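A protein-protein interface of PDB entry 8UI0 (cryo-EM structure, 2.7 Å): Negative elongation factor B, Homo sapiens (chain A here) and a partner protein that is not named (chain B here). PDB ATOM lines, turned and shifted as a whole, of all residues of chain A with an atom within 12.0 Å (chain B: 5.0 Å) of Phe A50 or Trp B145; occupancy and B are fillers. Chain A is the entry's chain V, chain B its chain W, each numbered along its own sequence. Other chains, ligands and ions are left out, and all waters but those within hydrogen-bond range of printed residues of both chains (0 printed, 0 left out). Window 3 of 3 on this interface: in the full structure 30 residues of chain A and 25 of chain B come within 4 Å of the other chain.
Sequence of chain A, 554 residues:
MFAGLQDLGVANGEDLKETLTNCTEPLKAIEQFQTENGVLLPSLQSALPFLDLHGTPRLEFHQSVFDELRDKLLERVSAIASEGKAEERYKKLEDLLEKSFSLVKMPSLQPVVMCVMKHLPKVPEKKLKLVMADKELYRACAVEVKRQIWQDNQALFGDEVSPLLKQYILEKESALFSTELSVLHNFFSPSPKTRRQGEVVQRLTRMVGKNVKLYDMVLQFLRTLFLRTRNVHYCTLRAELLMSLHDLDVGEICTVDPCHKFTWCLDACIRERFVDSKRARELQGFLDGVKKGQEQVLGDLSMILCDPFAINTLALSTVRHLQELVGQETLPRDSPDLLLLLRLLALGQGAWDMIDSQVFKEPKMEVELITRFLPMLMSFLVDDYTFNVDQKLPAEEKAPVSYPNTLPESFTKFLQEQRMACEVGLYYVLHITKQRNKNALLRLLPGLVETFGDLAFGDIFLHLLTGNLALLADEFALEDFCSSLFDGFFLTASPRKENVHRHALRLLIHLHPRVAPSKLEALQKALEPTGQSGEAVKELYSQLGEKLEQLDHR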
ATOM      1  N   GLN A  34      26.882  10.098  -1.738  1.00  0.00           N
ATOM      2  CA  GLN A  34      26.312   9.843  -0.417  1.00  0.00           C
ATOM      3  C   GLN A  34      27.217   8.935   0.404  1.00  0.00           C
ATOM      4  O   GLN A  34      27.402   9.153   1.608  1.00  0.00           O
ATOM      5  CB  GLN A  34      24.923   9.218  -0.556  1.00  0.00           C
ATOM      6  CG  GLN A  34      23.836  10.196  -0.990  1.00  0.00           C
ATOM      7  CD  GLN A  34      22.526   9.518  -1.376  1.00  0.00           C
ATOM      8  OE1 GLN A  34      21.879   9.920  -2.340  1.00  0.00           O
ATOM      9  NE2 GLN A  34      22.121   8.503  -0.615  1.00  0.00           N
ATOM     10  N   PRO A  42      30.648   1.029  10.587  1.00  0.00           N
ATOM     11  CA  PRO A  42      30.105  -0.089   9.799  1.00  0.00           C
ATOM     12  C   PRO A  42      28.664  -0.425  10.133  1.00  0.00           C
ATOM     13  O   PRO A  42      27.955  -0.950   9.266  1.00  0.00           O
ATOM     14  CB  PRO A  42      31.043  -1.260  10.141  1.00  0.00           C
ATOM     15  CG  PRO A  42      31.959  -0.764  11.237  1.00  0.00           C
ATOM     16  CD  PRO A  42      31.396   0.520  11.749  1.00  0.00           C
ATOM     17  N   SER A  43      28.206  -0.138  11.353  1.00  0.00           N
ATOM     18  CA  SER A  43      26.819  -0.409  11.706  1.00  0.00           C
ATOM     19  C   SER A  43      25.848   0.511  10.981  1.00  0.00           C
ATOM     20  O   SER A  43      24.685   0.138  10.795  1.00  0.00           O
ATOM     21  CB  SER A  43      26.624  -0.265  13.216  1.00  0.00           C
ATOM     22  OG  SER A  43      26.613   1.101  13.595  1.00  0.00           O
ATOM     23  N   LEU A  44      26.295   1.699  10.566  1.00  0.00           N
ATOM     24  CA  LEU A  44      25.375   2.665   9.980  1.00  0.00           C
ATOM     25  C   LEU A  44      25.004   2.307   8.547  1.00  0.00           C
ATOM     26  O   LEU A  44      23.849   2.479   8.157  1.00  0.00           O
ATOM     27  CB  LEU A  44      25.978   4.072  10.036  1.00  0.00           C
ATOM     28  CG  LEU A  44      26.190   4.740  11.403  1.00  0.00           C
ATOM     29  CD1 LEU A  44      26.597   6.182  11.194  1.00  0.00           C
ATOM     30  CD2 LEU A  44      24.957   4.682  12.301  1.00  0.00           C
ATOM     31  N   GLN A  45      25.942   1.781   7.752  1.00  0.00           N
ATOM     32  CA  GLN A  45      25.660   1.551   6.334  1.00  0.00           C
ATOM     33  C   GLN A  45      24.555   0.521   6.098  1.00  0.00           C
ATOM     34  O   GLN A  45      24.009   0.471   4.989  1.00  0.00           O
ATOM     35  CB  GLN A  45      26.935   1.119   5.601  1.00  0.00           C
ATOM     36  CG  GLN A  45      28.049   2.168   5.570  1.00  0.00           C
ATOM     37  CD  GLN A  45      27.655   3.430   4.817  1.00  0.00           C
ATOM     38  OE1 GLN A  45      26.942   3.372   3.816  1.00  0.00           O
ATOM     39  NE2 GLN A  45      28.121   4.578   5.298  1.00  0.00           N
ATOM     40  N   SER A  46      24.214  -0.290   7.100  1.00  0.00           N
ATOM     41  CA  SER A  46      23.034  -1.149   7.071  1.00  0.00           C
ATOM     42  C   SER A  46      21.825  -0.513   7.745  1.00  0.00           C
ATOM     43  O   SER A  46      20.694  -0.710   7.289  1.00  0.00           O
ATOM     44  CB  SER A  46      23.341  -2.488   7.748  1.00  0.00           C
ATOM     45  OG  SER A  46      23.781  -2.295   9.082  1.00  0.00           O
ATOM     46  N   ALA A  47      22.035   0.249   8.821  1.00  0.00           N
ATOM     47  CA  ALA A  47      20.934   0.857   9.560  1.00  0.00           C
ATOM     48  C   ALA A  47      20.321   2.057   8.847  1.00  0.00           C
ATOM     49  O   ALA A  47      19.187   2.432   9.165  1.00  0.00           O
ATOM     50  CB  ALA A  47      21.413   1.288  10.948  1.00  0.00           C
ATOM     51  N   LEU A  48      21.046   2.674   7.913  1.00  0.00           N
ATOM     52  CA  LEU A  48      20.551   3.880   7.252  1.00  0.00           C
ATOM     53  C   LEU A  48      19.283   3.620   6.445  1.00  0.00           C
ATOM     54  O   LEU A  48      18.324   4.399   6.586  1.00  0.00           O
ATOM     55  CB  LEU A  48      21.676   4.492   6.398  1.00  0.00           C
ATOM     56  CG  LEU A  48      22.884   5.266   6.979  1.00  0.00           C
ATOM     57  CD1 LEU A  48      23.406   6.302   5.998  1.00  0.00           C
ATOM     58  CD2 LEU A  48      22.622   5.930   8.326  1.00  0.00           C
ATOM     59  N   PRO A  49      19.192   2.579   5.599  1.00  0.00           N
ATOM     60  CA  PRO A  49      17.880   2.255   5.004  1.00  0.00           C
ATOM     61  C   PRO A  49      16.797   1.948   6.025  1.00  0.00           C
ATOM     62  O   PRO A  49      15.642   2.364   5.848  1.00  0.00           O
ATOM     63  CB  PRO A  49      18.184   1.025   4.138  1.00  0.00           C
ATOM     64  CG  PRO A  49      19.604   1.119   3.813  1.00  0.00           C
ATOM     65  CD  PRO A  49      20.282   1.826   4.946  1.00  0.00           C
ATOM     66  N   PHE A  50      17.139   1.230   7.097  1.00  0.00           N
ATOM     67  CA  PHE A  50      16.132   0.833   8.076  1.00  0.00           C
ATOM     68  C   PHE A  50      15.553   2.046   8.789  1.00  0.00           C
ATOM     69  O   PHE A  50      14.331   2.179   8.927  1.00  0.00           O
ATOM     70  CB  PHE A  50      16.734  -0.125   9.097  1.00  0.00           C
ATOM     71  CG  PHE A  50      15.873  -0.323  10.305  1.00  0.00           C
ATOM     72  CD1 PHE A  50      14.645  -0.953  10.195  1.00  0.00           C
ATOM     73  CD2 PHE A  50      16.260   0.167  11.541  1.00  0.00           C
ATOM     74  CE1 PHE A  50      13.840  -1.134  11.299  1.00  0.00           C
ATOM     75  CE2 PHE A  50      15.458  -0.012  12.653  1.00  0.00           C
ATOM     76  CZ  PHE A  50      14.246  -0.661  12.530  1.00  0.00           C
ATOM     77  N   LEU A  51      16.420   2.943   9.259  1.00  0.00           N
ATOM     78  CA  LEU A  51      15.938   4.152   9.912  1.00  0.00           C
ATOM     79  C   LEU A  51      15.281   5.092   8.910  1.00  0.00           C
ATOM     80  O   LEU A  51      14.399   5.874   9.283  1.00  0.00           O
ATOM     81  CB  LEU A  51      17.094   4.834  10.646  1.00  0.00           C
ATOM     82  CG  LEU A  51      16.834   6.152  11.384  1.00  0.00           C
ATOM     83  CD1 LEU A  51      15.942   5.925  12.591  1.00  0.00           C
ATOM     84  CD2 LEU A  51      18.156   6.758  11.809  1.00  0.00           C
ATOM     85  N   ASP A  52      15.691   5.032   7.639  1.00  0.00           N
ATOM     86  CA  ASP A  52      15.014   5.817   6.613  1.00  0.00           C
ATOM     87  C   ASP A  52      13.588   5.335   6.385  1.00  0.00           C
ATOM     88  O   ASP A  52      12.717   6.136   6.028  1.00  0.00           O
ATOM     89  CB  ASP A  52      15.802   5.762   5.300  1.00  0.00           C
ATOM     90  CG  ASP A  52      16.937   6.773   5.245  1.00  0.00           C
ATOM     91  OD1 ASP A  52      16.736   7.935   5.653  1.00  0.00           O
ATOM     92  OD2 ASP A  52      18.037   6.409   4.782  1.00  0.00           O
ATOM     93  N   LEU A  53      13.338   4.034   6.565  1.00  0.00           N
ATOM     94  CA  LEU A  53      11.990   3.499   6.377  1.00  0.00           C
ATOM     95  C   LEU A  53      10.986   4.127   7.343  1.00  0.00           C
ATOM     96  O   LEU A  53       9.798   4.229   7.018  1.00  0.00           O
ATOM     97  CB  LEU A  53      12.009   1.975   6.546  1.00  0.00           C
ATOM     98  CG  LEU A  53      10.718   1.147   6.439  1.00  0.00           C
ATOM     99  CD1 LEU A  53      10.445   0.764   4.994  1.00  0.00           C
ATOM    100  CD2 LEU A  53      10.809  -0.093   7.317  1.00  0.00           C
ATOM    101  N   HIS A  54      11.436   4.551   8.527  1.00  0.00           N
ATOM    102  CA  HIS A  54      10.534   5.068   9.554  1.00  0.00           C
ATOM    103  C   HIS A  54       9.912   6.415   9.209  1.00  0.00           C
ATOM    104  O   HIS A  54       8.979   6.832   9.906  1.00  0.00           O
ATOM    105  CB  HIS A  54      11.283   5.214  10.881  1.00  0.00           C
ATOM    106  CG  HIS A  54      11.760   3.919  11.459  1.00  0.00           C
ATOM    107  ND1 HIS A  54      12.635   3.860  12.521  1.00  0.00           N
ATOM    108  CD2 HIS A  54      11.478   2.636  11.132  1.00  0.00           C
ATOM    109  CE1 HIS A  54      12.877   2.596  12.820  1.00  0.00           C
ATOM    110  NE2 HIS A  54      12.188   1.833  11.992  1.00  0.00           N
ATOM    111  N   GLY A  55      10.388   7.099   8.173  1.00  0.00           N
ATOM    112  CA  GLY A  55      10.089   8.504   7.990  1.00  0.00           C
ATOM    113  C   GLY A  55      11.050   9.438   8.690  1.00  0.00           C
ATOM    114  O   GLY A  55      10.771  10.642   8.762  1.00  0.00           O
ATOM    115  N   THR A  56      12.171   8.920   9.213  1.00  0.00           N
ATOM    116  CA  THR A  56      13.225   9.720   9.819  1.00  0.00           C
ATOM    117  C   THR A  56      14.416   9.759   8.866  1.00  0.00           C
ATOM    118  O   THR A  56      15.045   8.711   8.654  1.00  0.00           O
ATOM    119  CB  THR A  56      13.643   9.120  11.159  1.00  0.00           C
ATOM    120  OG1 THR A  56      12.501   9.021  12.018  1.00  0.00           O
ATOM    121  CG2 THR A  56      14.714   9.977  11.825  1.00  0.00           C
ATOM    122  N   PRO A  57      14.773  10.896   8.263  1.00  0.00           N
ATOM    123  CA  PRO A  57      15.945  10.900   7.381  1.00  0.00           C
ATOM    124  C   PRO A  57      17.252  10.784   8.152  1.00  0.00           C
ATOM    125  O   PRO A  57      17.320  10.971   9.370  1.00  0.00           O
ATOM    126  CB  PRO A  57      15.830  12.240   6.651  1.00  0.00           C
ATOM    127  CG  PRO A  57      15.155  13.122   7.629  1.00  0.00           C
ATOM    128  CD  PRO A  57      14.160  12.239   8.325  1.00  0.00           C
ATOM    129  N   ARG A  58      18.301  10.438   7.397  1.00  0.00           N
ATOM    130  CA  ARG A  58      19.627  10.220   7.973  1.00  0.00           C
ATOM    131  C   ARG A  58      20.135  11.490   8.651  1.00  0.00           C
ATOM    132  O   ARG A  58      20.766  11.447   9.720  1.00  0.00           O
ATOM    133  CB  ARG A  58      20.591   9.768   6.861  1.00  0.00           C
ATOM    134  CG  ARG A  58      20.145   8.516   6.047  1.00  0.00           C
ATOM    135  CD  ARG A  58      20.850   8.406   4.686  1.00  0.00           C
ATOM    136  NE  ARG A  58      20.789   7.065   4.116  1.00  0.00           N
ATOM    137  CZ  ARG A  58      21.509   6.632   3.087  1.00  0.00           C
ATOM    138  NH1 ARG A  58      22.370   7.417   2.454  1.00  0.00           N
ATOM    139  NH2 ARG A  58      21.356   5.376   2.676  1.00  0.00           N
ATOM    140  N   LEU A  59      19.824  12.638   8.052  1.00  0.00           N
ATOM    141  CA  LEU A  59      20.205  13.935   8.592  1.00  0.00           C
ATOM    142  C   LEU A  59      19.642  14.189   9.985  1.00  0.00           C
ATOM    143  O   LEU A  59      20.174  15.036  10.698  1.00  0.00           O
ATOM    144  CB  LEU A  59      19.718  15.046   7.667  1.00  0.00           C
ATOM    145  CG  LEU A  59      18.204  15.043   7.402  1.00  0.00           C
ATOM    146  CD1 LEU A  59      17.395  15.930   8.389  1.00  0.00           C
ATOM    147  CD2 LEU A  59      17.917  15.277   5.939  1.00  0.00           C
ATOM    148  N   GLU A  60      18.569  13.502  10.388  1.00  0.00           N
ATOM    149  CA  GLU A  60      17.936  13.814  11.668  1.00  0.00           C
ATOM    150  C   GLU A  60      18.744  13.261  12.839  1.00  0.00           C
ATOM    151  O   GLU A  60      19.064  13.992  13.791  1.00  0.00           O
ATOM    152  CB  GLU A  60      16.506  13.271  11.686  1.00  0.00           C
ATOM    153  CG  GLU A  60      15.657  13.804  12.830  1.00  0.00           C
ATOM    154  CD  GLU A  60      14.174  13.584  12.605  1.00  0.00           C
ATOM    155  OE1 GLU A  60      13.662  14.013  11.548  1.00  0.00           O
ATOM    156  OE2 GLU A  60      13.518  12.984  13.482  1.00  0.00           O
ATOM    157  N   PHE A  61      19.097  11.972  12.788  1.00  0.00           N
ATOM    158  CA  PHE A  61      20.019  11.462  13.794  1.00  0.00           C
ATOM    159  C   PHE A  61      21.380  12.122  13.635  1.00  0.00           C
ATOM    160  O   PHE A  61      22.101  12.296  14.629  1.00  0.00           O
ATOM    161  CB  PHE A  61      20.105   9.923  13.747  1.00  0.00           C
ATOM    162  CG  PHE A  61      21.051   9.356  12.709  1.00  0.00           C
ATOM    163  CD1 PHE A  61      22.382   9.094  13.020  1.00  0.00           C
ATOM    164  CD2 PHE A  61      20.597   9.027  11.447  1.00  0.00           C
ATOM    165  CE1 PHE A  61      23.241   8.564  12.078  1.00  0.00           C
ATOM    166  CE2 PHE A  61      21.458   8.494  10.501  1.00  0.00           C
ATOM    167  CZ  PHE A  61      22.776   8.260  10.820  1.00  0.00           C
ATOM    168  N   HIS A  62      21.736  12.537  12.409  1.00  0.00           N
ATOM    169  CA  HIS A  62      22.938  13.354  12.273  1.00  0.00           C
ATOM    170  C   HIS A  62      22.811  14.668  13.045  1.00  0.00           C
ATOM    171  O   HIS A  62      23.769  15.116  13.665  1.00  0.00           O
ATOM    172  CB  HIS A  62      23.257  13.639  10.807  1.00  0.00           C
ATOM    173  CG  HIS A  62      23.613  12.424  10.007  1.00  0.00           C
ATOM    174  ND1 HIS A  62      23.183  12.238   8.710  1.00  0.00           N
ATOM    175  CD2 HIS A  62      24.360  11.337  10.314  1.00  0.00           C
ATOM    176  CE1 HIS A  62      23.651  11.089   8.254  1.00  0.00           C
ATOM    177  NE2 HIS A  62      24.364  10.522   9.209  1.00  0.00           N
ATOM    178  N   LEU B 123      13.470   4.967  19.609  1.00  0.00           N
ATOM    179  CA  LEU B 123      12.660   3.824  19.196  1.00  0.00           C
ATOM    180  C   LEU B 123      11.624   3.467  20.254  1.00  0.00           C
ATOM    181  O   LEU B 123      10.444   3.276  19.941  1.00  0.00           O
ATOM    182  CB  LEU B 123      13.561   2.622  18.912  1.00  0.00           C
ATOM    183  CG  LEU B 123      14.438   2.713  17.662  1.00  0.00           C
ATOM    184  CD1 LEU B 123      15.515   1.650  17.682  1.00  0.00           C
ATOM    185  CD2 LEU B 123      13.601   2.572  16.399  1.00  0.00           C
ATOM    186  N   ILE B 135       4.978  -5.085   9.994  1.00  0.00           N
ATOM    187  CA  ILE B 135       6.204  -5.727   9.523  1.00  0.00           C
ATOM    188  C   ILE B 135       6.017  -7.238   9.482  1.00  0.00           C
ATOM    189  O   ILE B 135       6.533  -7.920   8.590  1.00  0.00           O
ATOM    190  CB  ILE B 135       7.403  -5.328  10.409  1.00  0.00           C
ATOM    191  CG1 ILE B 135       7.757  -3.836  10.262  1.00  0.00           C
ATOM    192  CG2 ILE B 135       8.620  -6.210  10.116  1.00  0.00           C
ATOM    193  CD1 ILE B 135       8.314  -3.401   8.900  1.00  0.00           C
ATOM    194  N   THR B 142      11.077 -11.370   9.778  1.00  0.00           N
ATOM    195  CA  THR B 142      11.614 -10.035   9.566  1.00  0.00           C
ATOM    196  C   THR B 142      12.864 -10.123   8.690  1.00  0.00           C
ATOM    197  O   THR B 142      13.668 -11.047   8.865  1.00  0.00           O
ATOM    198  CB  THR B 142      11.965  -9.375  10.900  1.00  0.00           C
ATOM    199  OG1 THR B 142      12.730 -10.287  11.697  1.00  0.00           O
ATOM    200  CG2 THR B 142      10.709  -8.968  11.657  1.00  0.00           C
ATOM    201  N   PRO B 143      13.087  -9.172   7.742  1.00  0.00           N
ATOM    202  CA  PRO B 143      14.302  -9.263   6.914  1.00  0.00           C
ATOM    203  C   PRO B 143      15.589  -9.126   7.714  1.00  0.00           C
ATOM    204  O   PRO B 143      15.570  -9.003   8.943  1.00  0.00           O
ATOM    205  CB  PRO B 143      14.151  -8.105   5.919  1.00  0.00           C
ATOM    206  CG  PRO B 143      12.732  -7.798   5.890  1.00  0.00           C
ATOM    207  CD  PRO B 143      12.200  -8.097   7.256  1.00  0.00           C
ATOM    208  N   ALA B 144      16.721  -9.133   7.007  1.00  0.00           N
ATOM    209  CA  ALA B 144      18.028  -9.267   7.638  1.00  0.00           C
ATOM    210  C   ALA B 144      18.383  -8.117   8.576  1.00  0.00           C
ATOM    211  O   ALA B 144      19.368  -8.240   9.313  1.00  0.00           O
ATOM    212  CB  ALA B 144      19.107  -9.395   6.562  1.00  0.00           C
ATOM    213  N   TRP B 145      17.644  -7.002   8.562  1.00  0.00           N
ATOM    214  CA  TRP B 145      17.921  -5.948   9.535  1.00  0.00           C
ATOM    215  C   TRP B 145      17.681  -6.432  10.963  1.00  0.00           C
ATOM    216  O   TRP B 145      18.474  -6.129  11.861  1.00  0.00           O
ATOM    217  CB  TRP B 145      17.111  -4.675   9.244  1.00  0.00           C
ATOM    218  CG  TRP B 145      15.634  -4.817   8.968  1.00  0.00           C
ATOM    219  CD1 TRP B 145      15.054  -4.998   7.750  1.00  0.00           C
ATOM    220  CD2 TRP B 145      14.559  -4.747   9.917  1.00  0.00           C
ATOM    221  NE1 TRP B 145      13.690  -5.062   7.878  1.00  0.00           N
ATOM    222  CE2 TRP B 145      13.359  -4.910   9.197  1.00  0.00           C
ATOM    223  CE3 TRP B 145      14.493  -4.569  11.303  1.00  0.00           C
ATOM    224  CZ2 TRP B 145      12.111  -4.904   9.813  1.00  0.00           C
ATOM    225  CZ3 TRP B 145      13.249  -4.564  11.914  1.00  0.00           C
ATOM    226  CH2 TRP B 145      12.076  -4.730  11.168  1.00  0.00           C
ATOM    227  N   LEU B 146      16.615  -7.206  11.193  1.00  0.00           N
ATOM    228  CA  LEU B 146      16.388  -7.762  12.528  1.00  0.00           C
ATOM    229  C   LEU B 146      17.510  -8.716  12.920  1.00  0.00           C
ATOM    230  O   LEU B 146      18.038  -8.648  14.036  1.00  0.00           O
ATOM    231  CB  LEU B 146      15.039  -8.484  12.594  1.00  0.00           C
ATOM    232  CG  LEU B 146      14.703  -9.059  13.988  1.00  0.00           C
ATOM    233  CD1 LEU B 146      13.271  -8.762  14.451  1.00  0.00           C
ATOM    234  CD2 LEU B 146      14.964 -10.573  14.062  1.00  0.00           C
ATOM    235  N   GLU B 147      17.891  -9.615  12.009  1.00  0.00           N
ATOM    236  CA  GLU B 147      18.945 -10.580  12.301  1.00  0.00           C
ATOM    237  C   GLU B 147      20.324  -9.938  12.397  1.00  0.00           C
ATOM    238  O   GLU B 147      21.255 -10.592  12.878  1.00  0.00           O
ATOM    239  CB  GLU B 147      18.956 -11.676  11.235  1.00  0.00           C
ATOM    240  CG  GLU B 147      17.688 -12.518  11.213  1.00  0.00           C
ATOM    241  CD  GLU B 147      17.780 -13.693  10.260  1.00  0.00           C
ATOM    242  OE1 GLU B 147      18.669 -13.682   9.383  1.00  0.00           O
ATOM    243  OE2 GLU B 147      16.964 -14.630  10.389  1.00  0.00           O
ATOM    244  N   GLN B 148      20.478  -8.693  11.940  1.00  0.00           N
ATOM    245  CA  GLN B 148      21.692  -7.920  12.173  1.00  0.00           C
ATOM    246  C   GLN B 148      21.636  -7.150  13.484  1.00  0.00           C
ATOM    247  O   GLN B 148      22.680  -6.941  14.112  1.00  0.00           O
ATOM    248  CB  GLN B 148      21.923  -6.955  11.004  1.00  0.00           C
ATOM    249  CG  GLN B 148      23.374  -6.493  10.814  1.00  0.00           C
ATOM    250  CD  GLN B 148      23.784  -5.374  11.759  1.00  0.00           C
ATOM    251  OE1 GLN B 148      22.978  -4.511  12.109  1.00  0.00           O
ATOM    252  NE2 GLN B 148      25.046  -5.384  12.173  1.00  0.00           N
ATOM    253  N   MET B 149      20.445  -6.718  13.913  1.00  0.00           N
ATOM    254  CA  MET B 149      20.351  -6.000  15.178  1.00  0.00           C
ATOM    255  C   MET B 149      20.559  -6.940  16.360  1.00  0.00           C
ATOM    256  O   MET B 149      21.188  -6.562  17.356  1.00  0.00           O
ATOM    257  CB  MET B 149      19.002  -5.294  15.305  1.00  0.00           C
ATOM    258  CG  MET B 149      18.883  -4.044  14.461  1.00  0.00           C
ATOM    259  SD  MET B 149      17.294  -3.963  13.616  1.00  0.00           S
ATOM    260  CE  MET B 149      17.634  -2.695  12.415  1.00  0.00           C
ATOM    261  N   TRP B 155      20.245  -4.110  21.366  1.00  0.00           N
ATOM    262  CA  TRP B 155      19.039  -4.340  20.578  1.00  0.00           C
ATOM    263  C   TRP B 155      18.327  -5.619  21.003  1.00  0.00           C
ATOM    264  O   TRP B 155      17.099  -5.708  20.902  1.00  0.00           O
ATOM    265  CB  TRP B 155      19.381  -4.401  19.094  1.00  0.00           C
ATOM    266  CG  TRP B 155      19.753  -3.082  18.495  1.00  0.00           C
ATOM    267  CD1 TRP B 155      20.957  -2.446  18.593  1.00  0.00           C
ATOM    268  CD2 TRP B 155      18.916  -2.237  17.699  1.00  0.00           C
ATOM    269  NE1 TRP B 155      20.923  -1.260  17.903  1.00  0.00           N
ATOM    270  CE2 TRP B 155      19.681  -1.108  17.344  1.00  0.00           C
ATOM    271  CE3 TRP B 155      17.595  -2.324  17.250  1.00  0.00           C
ATOM    272  CZ2 TRP B 155      19.169  -0.076  16.565  1.00  0.00           C
ATOM    273  CZ3 TRP B 155      17.091  -1.301  16.472  1.00  0.00           C
ATOM    274  CH2 TRP B 155      17.879  -0.193  16.136  1.00  0.00           C
ATOM    275  N   MET B 171       4.930 -10.120  15.545  1.00  0.00           N
ATOM    276  CA  MET B 171       6.370  -9.900  15.414  1.00  0.00           C
ATOM    277  C   MET B 171       7.055 -10.034  16.766  1.00  0.00           C
ATOM    278  O   MET B 171       8.095 -10.688  16.885  1.00  0.00           O
ATOM    279  CB  MET B 171       6.648  -8.523  14.785  1.00  0.00           C
ATOM    280  CG  MET B 171       8.098  -7.970  14.917  1.00  0.00           C
ATOM    281  SD  MET B 171       8.288  -6.287  14.303  1.00  0.00           S
ATOM    282  CE  MET B 171      10.074  -6.177  14.210  1.00  0.00           C
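Hydrophobic or aromatic side chains of chain A that line the printed part of chain B: Phe A50 and His A54.
Printed residues of chain B that touch a printed residue of chain A: Leu B123, Trp B145, Gln B148 and Met B149.
Among the printed residues, 4 pairs touch across the chains.
Among the printed residues, no Asp or Glu carboxylate lies within 4 Å of a Lys or Arg side-chain nitrogen of the other chain.
Among the printed residues, pairs that only touch across the chains: Phe A50 with Met B149 (3.3 Å), Phe A50 with Trp B145 (3.5 Å), His A54 with Leu B123 (3.7 Å) and Ser A46 with Gln B148 (3.8 Å).
Ser A43 touches none of the printed residues of chain B.
Printed residues of chain B within 4 Å of Ser A46: Gln B148 (3.8 Å).
Of chain B, only Trp B145 and Met B149 come within 4 Å of Phe A50.
Of the printed residues of chain B, His A54 touches Leu B123.
Thr A56 touches none of the printed residues of chain B.
Of the printed residues of chain A, Leu B123 touches His A54.
No residue of chain A comes within 4 Å of Thr B142.
Pro B143 touches none of the printed residues of chain A.
No residue of chain A comes within 4 Å of Ala B144.
Trp B145 touches one residue of chain A.
No residue of chain A comes within 4 Å of Leu B146.
No residue of chain A comes within 4 Å of Glu B147.
Printed residues of chain A within 4 Å of Gln B148: Ser A46.
Met B149 touches just one residue of chain A: Phe A50.
The nearest printed residue of chain B that does not touch Ser A46 is Trp B145 (5.7 Å).
OG of Ser A46 is in hydrogen-bond range of O of Ser A43 (3.1 Å).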
